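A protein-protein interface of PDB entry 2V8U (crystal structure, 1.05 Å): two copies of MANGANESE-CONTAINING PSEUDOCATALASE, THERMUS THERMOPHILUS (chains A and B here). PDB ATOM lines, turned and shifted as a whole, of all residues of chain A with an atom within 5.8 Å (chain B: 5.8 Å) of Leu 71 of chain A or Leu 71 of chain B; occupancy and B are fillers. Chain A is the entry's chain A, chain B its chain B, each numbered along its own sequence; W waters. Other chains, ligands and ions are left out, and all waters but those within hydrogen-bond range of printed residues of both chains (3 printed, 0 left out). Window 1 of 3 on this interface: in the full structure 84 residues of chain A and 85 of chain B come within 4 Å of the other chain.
Leu 3 of chain A touches Thr 68 of chain B, and with the chains exchanged Thr 68 of chain A touches Leu 3 of chain B. Phe 48 of chain A touches Ile 74 of chain B, and with the chains exchanged Ile 74 of chain A touches Phe 48 of chain B. Phe 48 of chain A touches Glu 75 of chain B, and with the chains exchanged Glu 75 of chain A touches Phe 48 of chain B. Leu 71 of chain B touches its own counterpart, Leu 71 of chain A. Positions printed for both chains: 2, 3, 40, 44, 48, 66, 67, 68, 69, 70, 71, 72, 73, 74, 75 and 76. Of the 14 pairs that touch across the chains among the printed residues, 14 have their exchanged pair printed and touching as well.
N of Leu 3 of chain A lies within hydrogen-bond range of O of Leu 3 of chain B, at 2.9 Å.
O of Leu 3 of chain B touches CA of Phe 2 of chain A, 3.2 Å away. CG2 of Thr 68 of chain B touches O of Phe 2 of chain A (3.5 Å). Leu 71 of chain B touches Phe 2 of chain A (CB to CD1, 3.5 Å). CG2 of Thr 68 of chain B touches C of Leu 3 of chain A, 3.8 Å away. CE2 of Phe 48 of chain A touches CD1 of Ile 74 of chain B, at 3.9 Å. Phe 48 of chain A touches Glu 75 of chain B. CG2 of Thr 68 of chain A touches O of Phe 2 of chain B (3.5 Å). Leu 3 of chain B touches Thr 68 of chain A (C to CG2, 3.7 Å). Leu 71 of chain A touches Phe 2 of chain B. Phe 48 of chain B touches Glu 75 of chain A (CZ to CA, 3.6 Å).
Water W3 bridges the backbone carbonyl oxygen (O) of Leu 3 of chain A (2.6 Å) and the backbone NH (N) of Leu 3 of chain B (2.8 Å). Water W1 bridges O of Thr 68 of chain B (2.8 Å) and N of Phe 2 of chain A (2.9 Å). Water W2 lies within hydrogen-bond range of the backbone NH (N) of Phe 2 of chain B (2.8 Å), the backbone carbonyl oxygen (O) of Thr 68 of chain A (2.9 Å) and the backbone NH (N) of Gly 72 of chain A (3.4 Å).
Printed residues of chain A that touch a printed residue of chain B: Phe 2, Leu 3, Phe 48, Thr 68, Leu 71, Ile 74 and Glu 75. Hydrophobic or aromatic side chains of chain A within 4 Å of the printed part of chain B: Phe 2, Phe 48, Leu 71 and Ile 74. Of the 16 printed residues of chain B, 7 touch a printed residue of chain A. Hydrophobic or aromatic side chains of chain B within 4 Å of the printed part of chain A: Phe 2, Phe 48, Leu 71 and Ile 74. Among the printed residues, 14 pairs touch across the chains. Among the printed residues, no Asp or Glu carboxylate lies within 4 Å of a Lys or Arg side-chain nitrogen of the other chain.
Of chain B, only Phe 2 (3.5 Å) and Leu 71 (3.7 Å) come within 4 Å of Leu 71 of chain A. Leu 71 of chain B touches two residues of chain A. Of the printed residues of chain A, Ile 74 of chain B touches Phe 48. Of the printed residues of chain B, Phe 2 of chain A touches Leu 3, Thr 68 and Leu 71. Of the printed residues of chain B, Phe 48 of chain A touches Ile 74 and Glu 75. Met 44 of chain A touches none of the printed residues of chain B. The nearest residue of chain B that does not touch Leu 71 of chain A is Phe 48 of chain B (4.6 Å). The nearest residue of chain A that does not touch Leu 71 of chain B is Phe 48 of chain A (4.7 Å).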
ATOM      1  N   PHE A   2     -29.193  16.752   0.565  1.00  0.00           N
ATOM      2  CA  PHE A   2     -28.455  16.423   1.773  1.00  0.00           C
ATOM      3  C   PHE A   2     -28.957  15.147   2.384  1.00  0.00           C
ATOM      4  O   PHE A   2     -30.121  14.748   2.213  1.00  0.00           O
ATOM      5  CB  PHE A   2     -28.566  17.602   2.777  1.00  0.00           C
ATOM      6  CG  PHE A   2     -27.879  18.830   2.280  1.00  0.00           C
ATOM      7  CD1 PHE A   2     -28.525  19.714   1.400  1.00  0.00           C
ATOM      8  CD2 PHE A   2     -26.562  19.134   2.641  1.00  0.00           C
ATOM      9  CE1 PHE A   2     -27.878  20.809   0.884  1.00  0.00           C
ATOM     10  CE2 PHE A   2     -25.926  20.238   2.157  1.00  0.00           C
ATOM     11  CZ  PHE A   2     -26.581  21.070   1.266  1.00  0.00           C
ATOM     12  N   LEU A   3     -28.078  14.512   3.146  1.00  0.00           N
ATOM     13  CA  LEU A   3     -28.367  13.339   3.961  1.00  0.00           C
ATOM     14  C   LEU A   3     -27.969  13.628   5.394  1.00  0.00           C
ATOM     15  O   LEU A   3     -27.116  14.498   5.646  1.00  0.00           O
ATOM     16  CB  LEU A   3     -27.594  12.093   3.479  1.00  0.00           C
ATOM     17  CG  LEU A   3     -27.727  11.734   2.009  1.00  0.00           C
ATOM     18  CD1 LEU A   3     -26.784  10.589   1.645  1.00  0.00           C
ATOM     19  CD2 LEU A   3     -29.174  11.367   1.656  1.00  0.00           C
ATOM     20  N   LEU A  40     -22.286  28.535   8.631  1.00  0.00           N
ATOM     21  CA  LEU A  40     -23.178  27.675   7.850  1.00  0.00           C
ATOM     22  C   LEU A  40     -23.842  28.418   6.716  1.00  0.00           C
ATOM     23  O   LEU A  40     -23.768  28.001   5.555  1.00  0.00           O
ATOM     24  CB  LEU A  40     -24.227  27.053   8.772  1.00  0.00           C
ATOM     25  CG  LEU A  40     -25.358  26.351   8.028  1.00  0.00           C
ATOM     26  CD1 LEU A  40     -24.872  25.184   7.210  1.00  0.00           C
ATOM     27  CD2 LEU A  40     -26.408  25.907   9.048  1.00  0.00           C
ATOM     28  N   MET A  44     -23.330  28.082   2.743  1.00  0.00           N
ATOM     29  CA  MET A  44     -24.439  27.421   2.058  1.00  0.00           C
ATOM     30  C   MET A  44     -24.925  28.309   0.907  1.00  0.00           C
ATOM     31  O   MET A  44     -25.017  27.848  -0.247  1.00  0.00           O
ATOM     32  CB  MET A  44     -25.560  27.123   3.035  1.00  0.00           C
ATOM     33  CG  MET A  44     -26.612  26.232   2.505  1.00  0.00           C
ATOM     34  SD  MET A  44     -26.077  24.586   2.067  1.00  0.00           S
ATOM     35  CE  MET A  44     -25.801  23.950   3.550  1.00  0.00           C
ATOM     36  N   PHE A  48     -24.770  27.840  -3.230  1.00  0.00           N
ATOM     37  CA  PHE A  48     -25.894  27.881  -4.149  1.00  0.00           C
ATOM     38  C   PHE A  48     -25.608  28.883  -5.272  1.00  0.00           C
ATOM     39  O   PHE A  48     -25.888  28.625  -6.461  1.00  0.00           O
ATOM     40  CB  PHE A  48     -27.180  28.307  -3.435  1.00  0.00           C
ATOM     41  CG  PHE A  48     -27.642  27.404  -2.290  1.00  0.00           C
ATOM     42  CD1 PHE A  48     -27.231  26.077  -2.165  1.00  0.00           C
ATOM     43  CD2 PHE A  48     -28.531  27.893  -1.360  1.00  0.00           C
ATOM     44  CE1 PHE A  48     -27.714  25.287  -1.143  1.00  0.00           C
ATOM     45  CE2 PHE A  48     -29.012  27.092  -0.343  1.00  0.00           C
ATOM     46  CZ  PHE A  48     -28.616  25.799  -0.231  1.00  0.00           C
ATOM     47  N   ILE A  66     -17.384  22.680   2.981  1.00  0.00           N
ATOM     48  CA  ILE A  66     -17.311  23.291   4.297  1.00  0.00           C
ATOM     49  C   ILE A  66     -18.722  23.665   4.774  1.00  0.00           C
ATOM     50  O   ILE A  66     -19.044  23.485   5.951  1.00  0.00           O
ATOM     51  CB  ILE A  66     -16.288  24.417   4.363  1.00  0.00           C
ATOM     52  CG1 ILE A  66     -14.862  23.864   4.154  1.00  0.00           C
ATOM     53  CG2 ILE A  66     -16.375  25.135   5.698  1.00  0.00           C
ATOM     54  CD1 ILE A  66     -13.797  24.954   4.057  1.00  0.00           C
ATOM     55  N   ALA A  67     -19.575  24.161   3.892  1.00  0.00           N
ATOM     56  CA  ALA A  67     -20.976  24.421   4.261  1.00  0.00           C
ATOM     57  C   ALA A  67     -21.596  23.194   4.917  1.00  0.00           C
ATOM     58  O   ALA A  67     -22.320  23.292   5.915  1.00  0.00           O
ATOM     59  CB  ALA A  67     -21.800  24.815   3.047  1.00  0.00           C
ATOM     60  N   THR A  68     -21.356  22.011   4.330  1.00  0.00           N
ATOM     61  CA  THR A  68     -21.927  20.782   4.852  1.00  0.00           C
ATOM     62  C   THR A  68     -21.378  20.469   6.244  1.00  0.00           C
ATOM     63  O   THR A  68     -22.116  20.053   7.141  1.00  0.00           O
ATOM     64  CB  THR A  68     -21.675  19.627   3.896  1.00  0.00           C
ATOM     65  OG1 THR A  68     -22.092  20.032   2.597  1.00  0.00           O
ATOM     66  CG2 THR A  68     -22.451  18.402   4.311  1.00  0.00           C
ATOM     67  N   GLU A  69     -20.078  20.649   6.451  1.00  0.00           N
ATOM     68  CA  GLU A  69     -19.531  20.467   7.797  1.00  0.00           C
ATOM     69  C   GLU A  69     -20.203  21.392   8.803  1.00  0.00           C
ATOM     70  O   GLU A  69     -20.502  20.996   9.939  1.00  0.00           O
ATOM     71  CB  GLU A  69     -18.007  20.702   7.823  1.00  0.00           C
ATOM     72  CG  GLU A  69     -17.473  20.449   9.233  1.00  0.00           C
ATOM     73  CD  GLU A  69     -15.985  20.474   9.448  1.00  0.00           C
ATOM     74  OE1 GLU A  69     -15.200  20.663   8.485  1.00  0.00           O
ATOM     75  OE2 GLU A  69     -15.597  20.294  10.637  1.00  0.00           O
ATOM     76  N   GLU A  70     -20.494  22.635   8.421  1.00  0.00           N
ATOM     77  CA  GLU A  70     -21.088  23.585   9.366  1.00  0.00           C
ATOM     78  C   GLU A  70     -22.465  23.152   9.821  1.00  0.00           C
ATOM     79  O   GLU A  70     -22.893  23.549  10.911  1.00  0.00           O
ATOM     80  CB  GLU A  70     -21.150  25.004   8.771  1.00  0.00           C
ATOM     81  CG  GLU A  70     -19.819  25.631   8.331  1.00  0.00           C
ATOM     82  CD  GLU A  70     -18.782  25.859   9.364  1.00  0.00           C
ATOM     83  OE1 GLU A  70     -18.946  25.423  10.521  1.00  0.00           O
ATOM     84  OE2 GLU A  70     -17.732  26.449   9.027  1.00  0.00           O
ATOM     85  N   LEU A  71     -23.195  22.355   9.035  1.00  0.00           N
ATOM     86  CA  LEU A  71     -24.457  21.796   9.529  1.00  0.00           C
ATOM     87  C   LEU A  71     -24.260  21.009  10.804  1.00  0.00           C
ATOM     88  O   LEU A  71     -25.043  21.091  11.760  1.00  0.00           O
ATOM     89  CB  LEU A  71     -25.101  20.879   8.475  1.00  0.00           C
ATOM     90  CG  LEU A  71     -25.671  21.603   7.246  1.00  0.00           C
ATOM     91  CD1 LEU A  71     -25.928  20.587   6.133  1.00  0.00           C
ATOM     92  CD2 LEU A  71     -26.953  22.323   7.610  1.00  0.00           C
ATOM     93  N   GLY A  72     -23.187  20.198  10.850  1.00  0.00           N
ATOM     94  CA  GLY A  72     -22.876  19.456  12.049  1.00  0.00           C
ATOM     95  C   GLY A  72     -22.379  20.347  13.174  1.00  0.00           C
ATOM     96  O   GLY A  72     -22.451  19.972  14.351  1.00  0.00           O
ATOM     97  N   HIS A  73     -21.870  21.542  12.860  1.00  0.00           N
ATOM     98  CA  HIS A  73     -21.454  22.470  13.894  1.00  0.00           C
ATOM     99  C   HIS A  73     -22.627  23.143  14.570  1.00  0.00           C
ATOM    100  O   HIS A  73     -22.629  23.279  15.795  1.00  0.00           O
ATOM    101  CB  HIS A  73     -20.481  23.496  13.277  1.00  0.00           C
ATOM    102  CG  HIS A  73     -19.154  22.885  12.990  1.00  0.00           C
ATOM    103  ND1 HIS A  73     -18.036  23.635  12.808  1.00  0.00           N
ATOM    104  CD2 HIS A  73     -18.802  21.596  12.835  1.00  0.00           C
ATOM    105  CE1 HIS A  73     -16.924  22.823  12.811  1.00  0.00           C
ATOM    106  NE2 HIS A  73     -17.450  21.576  12.606  1.00  0.00           N
ATOM    107  N   ILE A  74     -23.652  23.572  13.822  1.00  0.00           N
ATOM    108  CA  ILE A  74     -24.842  24.082  14.520  1.00  0.00           C
ATOM    109  C   ILE A  74     -25.412  22.991  15.403  1.00  0.00           C
ATOM    110  O   ILE A  74     -25.876  23.251  16.518  1.00  0.00           O
ATOM    111  CB  ILE A  74     -25.918  24.735  13.614  1.00  0.00           C
ATOM    112  CG1 ILE A  74     -26.559  23.809  12.598  1.00  0.00           C
ATOM    113  CG2 ILE A  74     -25.346  25.976  12.944  1.00  0.00           C
ATOM    114  CD1 ILE A  74     -27.884  24.333  12.036  1.00  0.00           C
ATOM    115  N   GLU A  75     -25.398  21.734  14.924  1.00  0.00           N
ATOM    116  CA  GLU A  75     -25.901  20.605  15.691  1.00  0.00           C
ATOM    117  C   GLU A  75     -25.106  20.454  16.977  1.00  0.00           C
ATOM    118  O   GLU A  75     -25.664  20.238  18.066  1.00  0.00           O
ATOM    119  CB  GLU A  75     -25.800  19.350  14.824  1.00  0.00           C
ATOM    120  CG  GLU A  75     -26.359  18.115  15.474  1.00  0.00           C
ATOM    121  CD  GLU A  75     -26.162  16.840  14.661  1.00  0.00           C
ATOM    122  OE1 GLU A  75     -25.316  16.845  13.712  1.00  0.00           O
ATOM    123  OE2 GLU A  75     -26.852  15.845  14.995  1.00  0.00           O
ATOM    124  N   LEU A  76     -23.773  20.509  16.896  1.00  0.00           N
ATOM    125  CA  LEU A  76     -22.916  20.325  18.064  1.00  0.00           C
ATOM    126  C   LEU A  76     -23.065  21.433  19.086  1.00  0.00           C
ATOM    127  O   LEU A  76     -23.114  21.175  20.308  1.00  0.00           O
ATOM    128  CB  LEU A  76     -21.462  20.201  17.604  1.00  0.00           C
ATOM    129  CG  LEU A  76     -20.461  19.826  18.690  1.00  0.00           C
ATOM    130  CD1 LEU A  76     -20.698  18.396  19.176  1.00  0.00           C
ATOM    131  CD2 LEU A  76     -19.033  19.968  18.191  1.00  0.00           C
ATOM    132  N   PHE B   2     -24.080  15.680   8.678  1.00  0.00           N
ATOM    133  CA  PHE B   2     -24.747  15.715   7.393  1.00  0.00           C
ATOM    134  C   PHE B   2     -23.763  15.424   6.268  1.00  0.00           C
ATOM    135  O   PHE B   2     -22.559  15.650   6.389  1.00  0.00           O
ATOM    136  CB  PHE B   2     -25.429  17.092   7.173  1.00  0.00           C
ATOM    137  CG  PHE B   2     -26.533  17.332   8.175  1.00  0.00           C
ATOM    138  CD1 PHE B   2     -26.268  17.780   9.453  1.00  0.00           C
ATOM    139  CD2 PHE B   2     -27.834  17.075   7.827  1.00  0.00           C
ATOM    140  CE1 PHE B   2     -27.308  17.939  10.381  1.00  0.00           C
ATOM    141  CE2 PHE B   2     -28.877  17.266   8.741  1.00  0.00           C
ATOM    142  CZ  PHE B   2     -28.606  17.680  10.010  1.00  0.00           C
ATOM    143  N   LEU B   3     -24.319  14.947   5.156  1.00  0.00           N
ATOM    144  CA  LEU B   3     -23.632  14.755   3.890  1.00  0.00           C
ATOM    145  C   LEU B   3     -24.347  15.546   2.828  1.00  0.00           C
ATOM    146  O   LEU B   3     -25.537  15.836   2.939  1.00  0.00           O
ATOM    147  CB  LEU B   3     -23.551  13.278   3.489  1.00  0.00           C
ATOM    148  CG  LEU B   3     -22.991  12.309   4.515  1.00  0.00           C
ATOM    149  CD1 LEU B   3     -23.166  10.879   4.027  1.00  0.00           C
ATOM    150  CD2 LEU B   3     -21.527  12.601   4.830  1.00  0.00           C
ATOM    151  N   LEU B  40     -37.265  24.472   7.204  1.00  0.00           N
ATOM    152  CA  LEU B  40     -35.952  23.913   7.515  1.00  0.00           C
ATOM    153  C   LEU B  40     -35.570  24.155   8.969  1.00  0.00           C
ATOM    154  O   LEU B  40     -35.229  23.213   9.692  1.00  0.00           O
ATOM    155  CB  LEU B  40     -34.876  24.538   6.602  1.00  0.00           C
ATOM    156  CG  LEU B  40     -33.435  24.244   7.017  1.00  0.00           C
ATOM    157  CD1 LEU B  40     -33.124  22.767   7.009  1.00  0.00           C
ATOM    158  CD2 LEU B  40     -32.496  25.022   6.112  1.00  0.00           C
ATOM    159  N   MET B  44     -35.188  21.551  11.988  1.00  0.00           N
ATOM    160  CA  MET B  44     -33.811  21.304  12.390  1.00  0.00           C
ATOM    161  C   MET B  44     -33.658  21.526  13.886  1.00  0.00           C
ATOM    162  O   MET B  44     -33.140  20.652  14.609  1.00  0.00           O
ATOM    163  CB  MET B  44     -32.866  22.193  11.596  1.00  0.00           C
ATOM    164  CG  MET B  44     -31.443  21.817  11.737  1.00  0.00           C
ATOM    165  SD  MET B  44     -30.985  20.194  11.127  1.00  0.00           S
ATOM    166  CE  MET B  44     -31.097  20.416   9.490  1.00  0.00           C
ATOM    167  N   PHE B  48     -32.837  18.904  17.009  1.00  0.00           N
ATOM    168  CA  PHE B  48     -31.767  19.024  17.982  1.00  0.00           C
ATOM    169  C   PHE B  48     -32.318  18.936  19.406  1.00  0.00           C
ATOM    170  O   PHE B  48     -31.764  18.252  20.289  1.00  0.00           O
ATOM    171  CB  PHE B  48     -31.006  20.343  17.823  1.00  0.00           C
ATOM    172  CG  PHE B  48     -30.349  20.572  16.469  1.00  0.00           C
ATOM    173  CD1 PHE B  48     -30.028  19.557  15.607  1.00  0.00           C
ATOM    174  CD2 PHE B  48     -30.015  21.866  16.130  1.00  0.00           C
ATOM    175  CE1 PHE B  48     -29.408  19.797  14.385  1.00  0.00           C
ATOM    176  CE2 PHE B  48     -29.357  22.124  14.928  1.00  0.00           C
ATOM    177  CZ  PHE B  48     -29.040  21.088  14.080  1.00  0.00           C
ATOM    178  N   ILE B  66     -37.515  15.014   7.945  1.00  0.00           N
ATOM    179  CA  ILE B  66     -38.103  16.097   7.170  1.00  0.00           C
ATOM    180  C   ILE B  66     -37.178  17.330   7.198  1.00  0.00           C
ATOM    181  O   ILE B  66     -37.006  17.998   6.180  1.00  0.00           O
ATOM    182  CB  ILE B  66     -39.559  16.381   7.555  1.00  0.00           C
ATOM    183  CG1 ILE B  66     -40.429  15.155   7.241  1.00  0.00           C
ATOM    184  CG2 ILE B  66     -40.081  17.594   6.807  1.00  0.00           C
ATOM    185  CD1 ILE B  66     -41.859  15.286   7.661  1.00  0.00           C
ATOM    186  N   ALA B  67     -36.552  17.624   8.346  1.00  0.00           N
ATOM    187  CA  ALA B  67     -35.568  18.703   8.393  1.00  0.00           C
ATOM    188  C   ALA B  67     -34.541  18.551   7.291  1.00  0.00           C
ATOM    189  O   ALA B  67     -34.130  19.526   6.650  1.00  0.00           O
ATOM    190  CB  ALA B  67     -34.867  18.733   9.755  1.00  0.00           C
ATOM    191  N   THR B  68     -34.058  17.322   7.104  1.00  0.00           N
ATOM    192  CA  THR B  68     -33.022  17.055   6.113  1.00  0.00           C
ATOM    193  C   THR B  68     -33.553  17.296   4.685  1.00  0.00           C
ATOM    194  O   THR B  68     -32.853  17.875   3.853  1.00  0.00           O
ATOM    195  CB  THR B  68     -32.485  15.646   6.274  1.00  0.00           C
ATOM    196  OG1 THR B  68     -32.104  15.448   7.642  1.00  0.00           O
ATOM    197  CG2 THR B  68     -31.274  15.416   5.398  1.00  0.00           C
ATOM    198  N   GLU B  69     -34.787  16.877   4.409  1.00  0.00           N
ATOM    199  CA  GLU B  69     -35.378  17.194   3.113  1.00  0.00           C
ATOM    200  C   GLU B  69     -35.402  18.705   2.878  1.00  0.00           C
ATOM    201  O   GLU B  69     -35.134  19.189   1.756  1.00  0.00           O
ATOM    202  CB  GLU B  69     -36.774  16.611   2.951  1.00  0.00           C
ATOM    203  CG  GLU B  69     -37.310  16.899   1.550  1.00  0.00           C
ATOM    204  CD  GLU B  69     -38.602  16.264   1.123  1.00  0.00           C
ATOM    205  OE1 GLU B  69     -39.220  15.517   1.888  1.00  0.00           O
ATOM    206  OE2 GLU B  69     -39.000  16.560  -0.057  1.00  0.00           O
ATOM    207  N   GLU B  70     -35.755  19.478   3.906  1.00  0.00           N
ATOM    208  CA  GLU B  70     -35.892  20.929   3.719  1.00  0.00           C
ATOM    209  C   GLU B  70     -34.570  21.587   3.344  1.00  0.00           C
ATOM    210  O   GLU B  70     -34.581  22.636   2.722  1.00  0.00           O
ATOM    211  CB  GLU B  70     -36.465  21.604   4.968  1.00  0.00           C
ATOM    212  CG  GLU B  70     -37.813  21.103   5.461  1.00  0.00           C
ATOM    213  CD  GLU B  70     -39.006  21.295   4.567  1.00  0.00           C
ATOM    214  OE1 GLU B  70     -38.819  21.703   3.397  1.00  0.00           O
ATOM    215  OE2 GLU B  70     -40.114  20.977   4.990  1.00  0.00           O
ATOM    216  N   LEU B  71     -33.415  20.994   3.674  1.00  0.00           N
ATOM    217  CA  LEU B  71     -32.130  21.504   3.182  1.00  0.00           C
ATOM    218  C   LEU B  71     -32.125  21.540   1.668  1.00  0.00           C
ATOM    219  O   LEU B  71     -31.639  22.497   1.048  1.00  0.00           O
ATOM    220  CB  LEU B  71     -30.972  20.655   3.693  1.00  0.00           C
ATOM    221  CG  LEU B  71     -30.634  20.785   5.179  1.00  0.00           C
ATOM    222  CD1 LEU B  71     -29.724  19.630   5.599  1.00  0.00           C
ATOM    223  CD2 LEU B  71     -29.979  22.116   5.469  1.00  0.00           C
ATOM    224  N   GLY B  72     -32.612  20.474   1.029  1.00  0.00           N
ATOM    225  CA  GLY B  72     -32.689  20.471  -0.411  1.00  0.00           C
ATOM    226  C   GLY B  72     -33.731  21.417  -0.956  1.00  0.00           C
ATOM    227  O   GLY B  72     -33.659  21.826  -2.110  1.00  0.00           O
ATOM    228  N   HIS B  73     -34.740  21.768  -0.148  1.00  0.00           N
ATOM    229  CA  HIS B  73     -35.736  22.736  -0.598  1.00  0.00           C
ATOM    230  C   HIS B  73     -35.178  24.160  -0.589  1.00  0.00           C
ATOM    231  O   HIS B  73     -35.462  24.906  -1.537  1.00  0.00           O
ATOM    232  CB  HIS B  73     -37.004  22.649   0.210  1.00  0.00           C
ATOM    233  CG  HIS B  73     -37.757  21.367   0.046  1.00  0.00           C
ATOM    234  ND1 HIS B  73     -38.997  21.184   0.569  1.00  0.00           N
ATOM    235  CD2 HIS B  73     -37.389  20.216  -0.603  1.00  0.00           C
ATOM    236  CE1 HIS B  73     -39.366  19.988   0.232  1.00  0.00           C
ATOM    237  NE2 HIS B  73     -38.426  19.365  -0.467  1.00  0.00           N
ATOM    238  N   ILE B  74     -34.402  24.576   0.429  1.00  0.00           N
ATOM    239  CA  ILE B  74     -33.784  25.892   0.314  1.00  0.00           C
ATOM    240  C   ILE B  74     -32.880  25.930  -0.903  1.00  0.00           C
ATOM    241  O   ILE B  74     -32.806  26.927  -1.608  1.00  0.00           O
ATOM    242  CB  ILE B  74     -33.077  26.397   1.604  1.00  0.00           C
ATOM    243  CG1 ILE B  74     -31.882  25.560   2.041  1.00  0.00           C
ATOM    244  CG2 ILE B  74     -34.072  26.590   2.738  1.00  0.00           C
ATOM    245  CD1 ILE B  74     -30.942  26.318   3.015  1.00  0.00           C
ATOM    246  N   GLU B  75     -32.175  24.812  -1.168  1.00  0.00           N
ATOM    247  CA  GLU B  75     -31.301  24.730  -2.337  1.00  0.00           C
ATOM    248  C   GLU B  75     -32.108  24.908  -3.631  1.00  0.00           C
ATOM    249  O   GLU B  75     -31.680  25.633  -4.543  1.00  0.00           O
ATOM    250  CB  GLU B  75     -30.586  23.363  -2.297  1.00  0.00           C
ATOM    251  CG  GLU B  75     -29.606  23.167  -3.405  1.00  0.00           C
ATOM    252  CD  GLU B  75     -28.954  21.794  -3.437  1.00  0.00           C
ATOM    253  OE1 GLU B  75     -29.503  20.841  -2.784  1.00  0.00           O
ATOM    254  OE2 GLU B  75     -27.920  21.667  -4.112  1.00  0.00           O
ATOM    255  N   LEU B  76     -33.244  24.239  -3.725  1.00  0.00           N
ATOM    256  CA  LEU B  76     -34.060  24.281  -4.942  1.00  0.00           C
ATOM    257  C   LEU B  76     -34.640  25.663  -5.162  1.00  0.00           C
ATOM    258  O   LEU B  76     -34.697  26.172  -6.293  1.00  0.00           O
ATOM    259  CB  LEU B  76     -35.147  23.227  -4.867  1.00  0.00           C
ATOM    260  CG  LEU B  76     -35.953  22.987  -6.126  1.00  0.00           C
ATOM    261  CD1 LEU B  76     -35.087  22.366  -7.202  1.00  0.00           C
ATOM    262  CD2 LEU B  76     -37.182  22.127  -5.856  1.00  0.00           C
HETATM  263  O   HOH W   1     -31.995  16.951   1.326  1.00  0.00           O
HETATM  264  O   HOH W   2     -22.061  17.682   8.785  1.00  0.00           O
HETATM  265  O   HOH W   3     -25.360  12.755   6.587  1.00  0.00           O
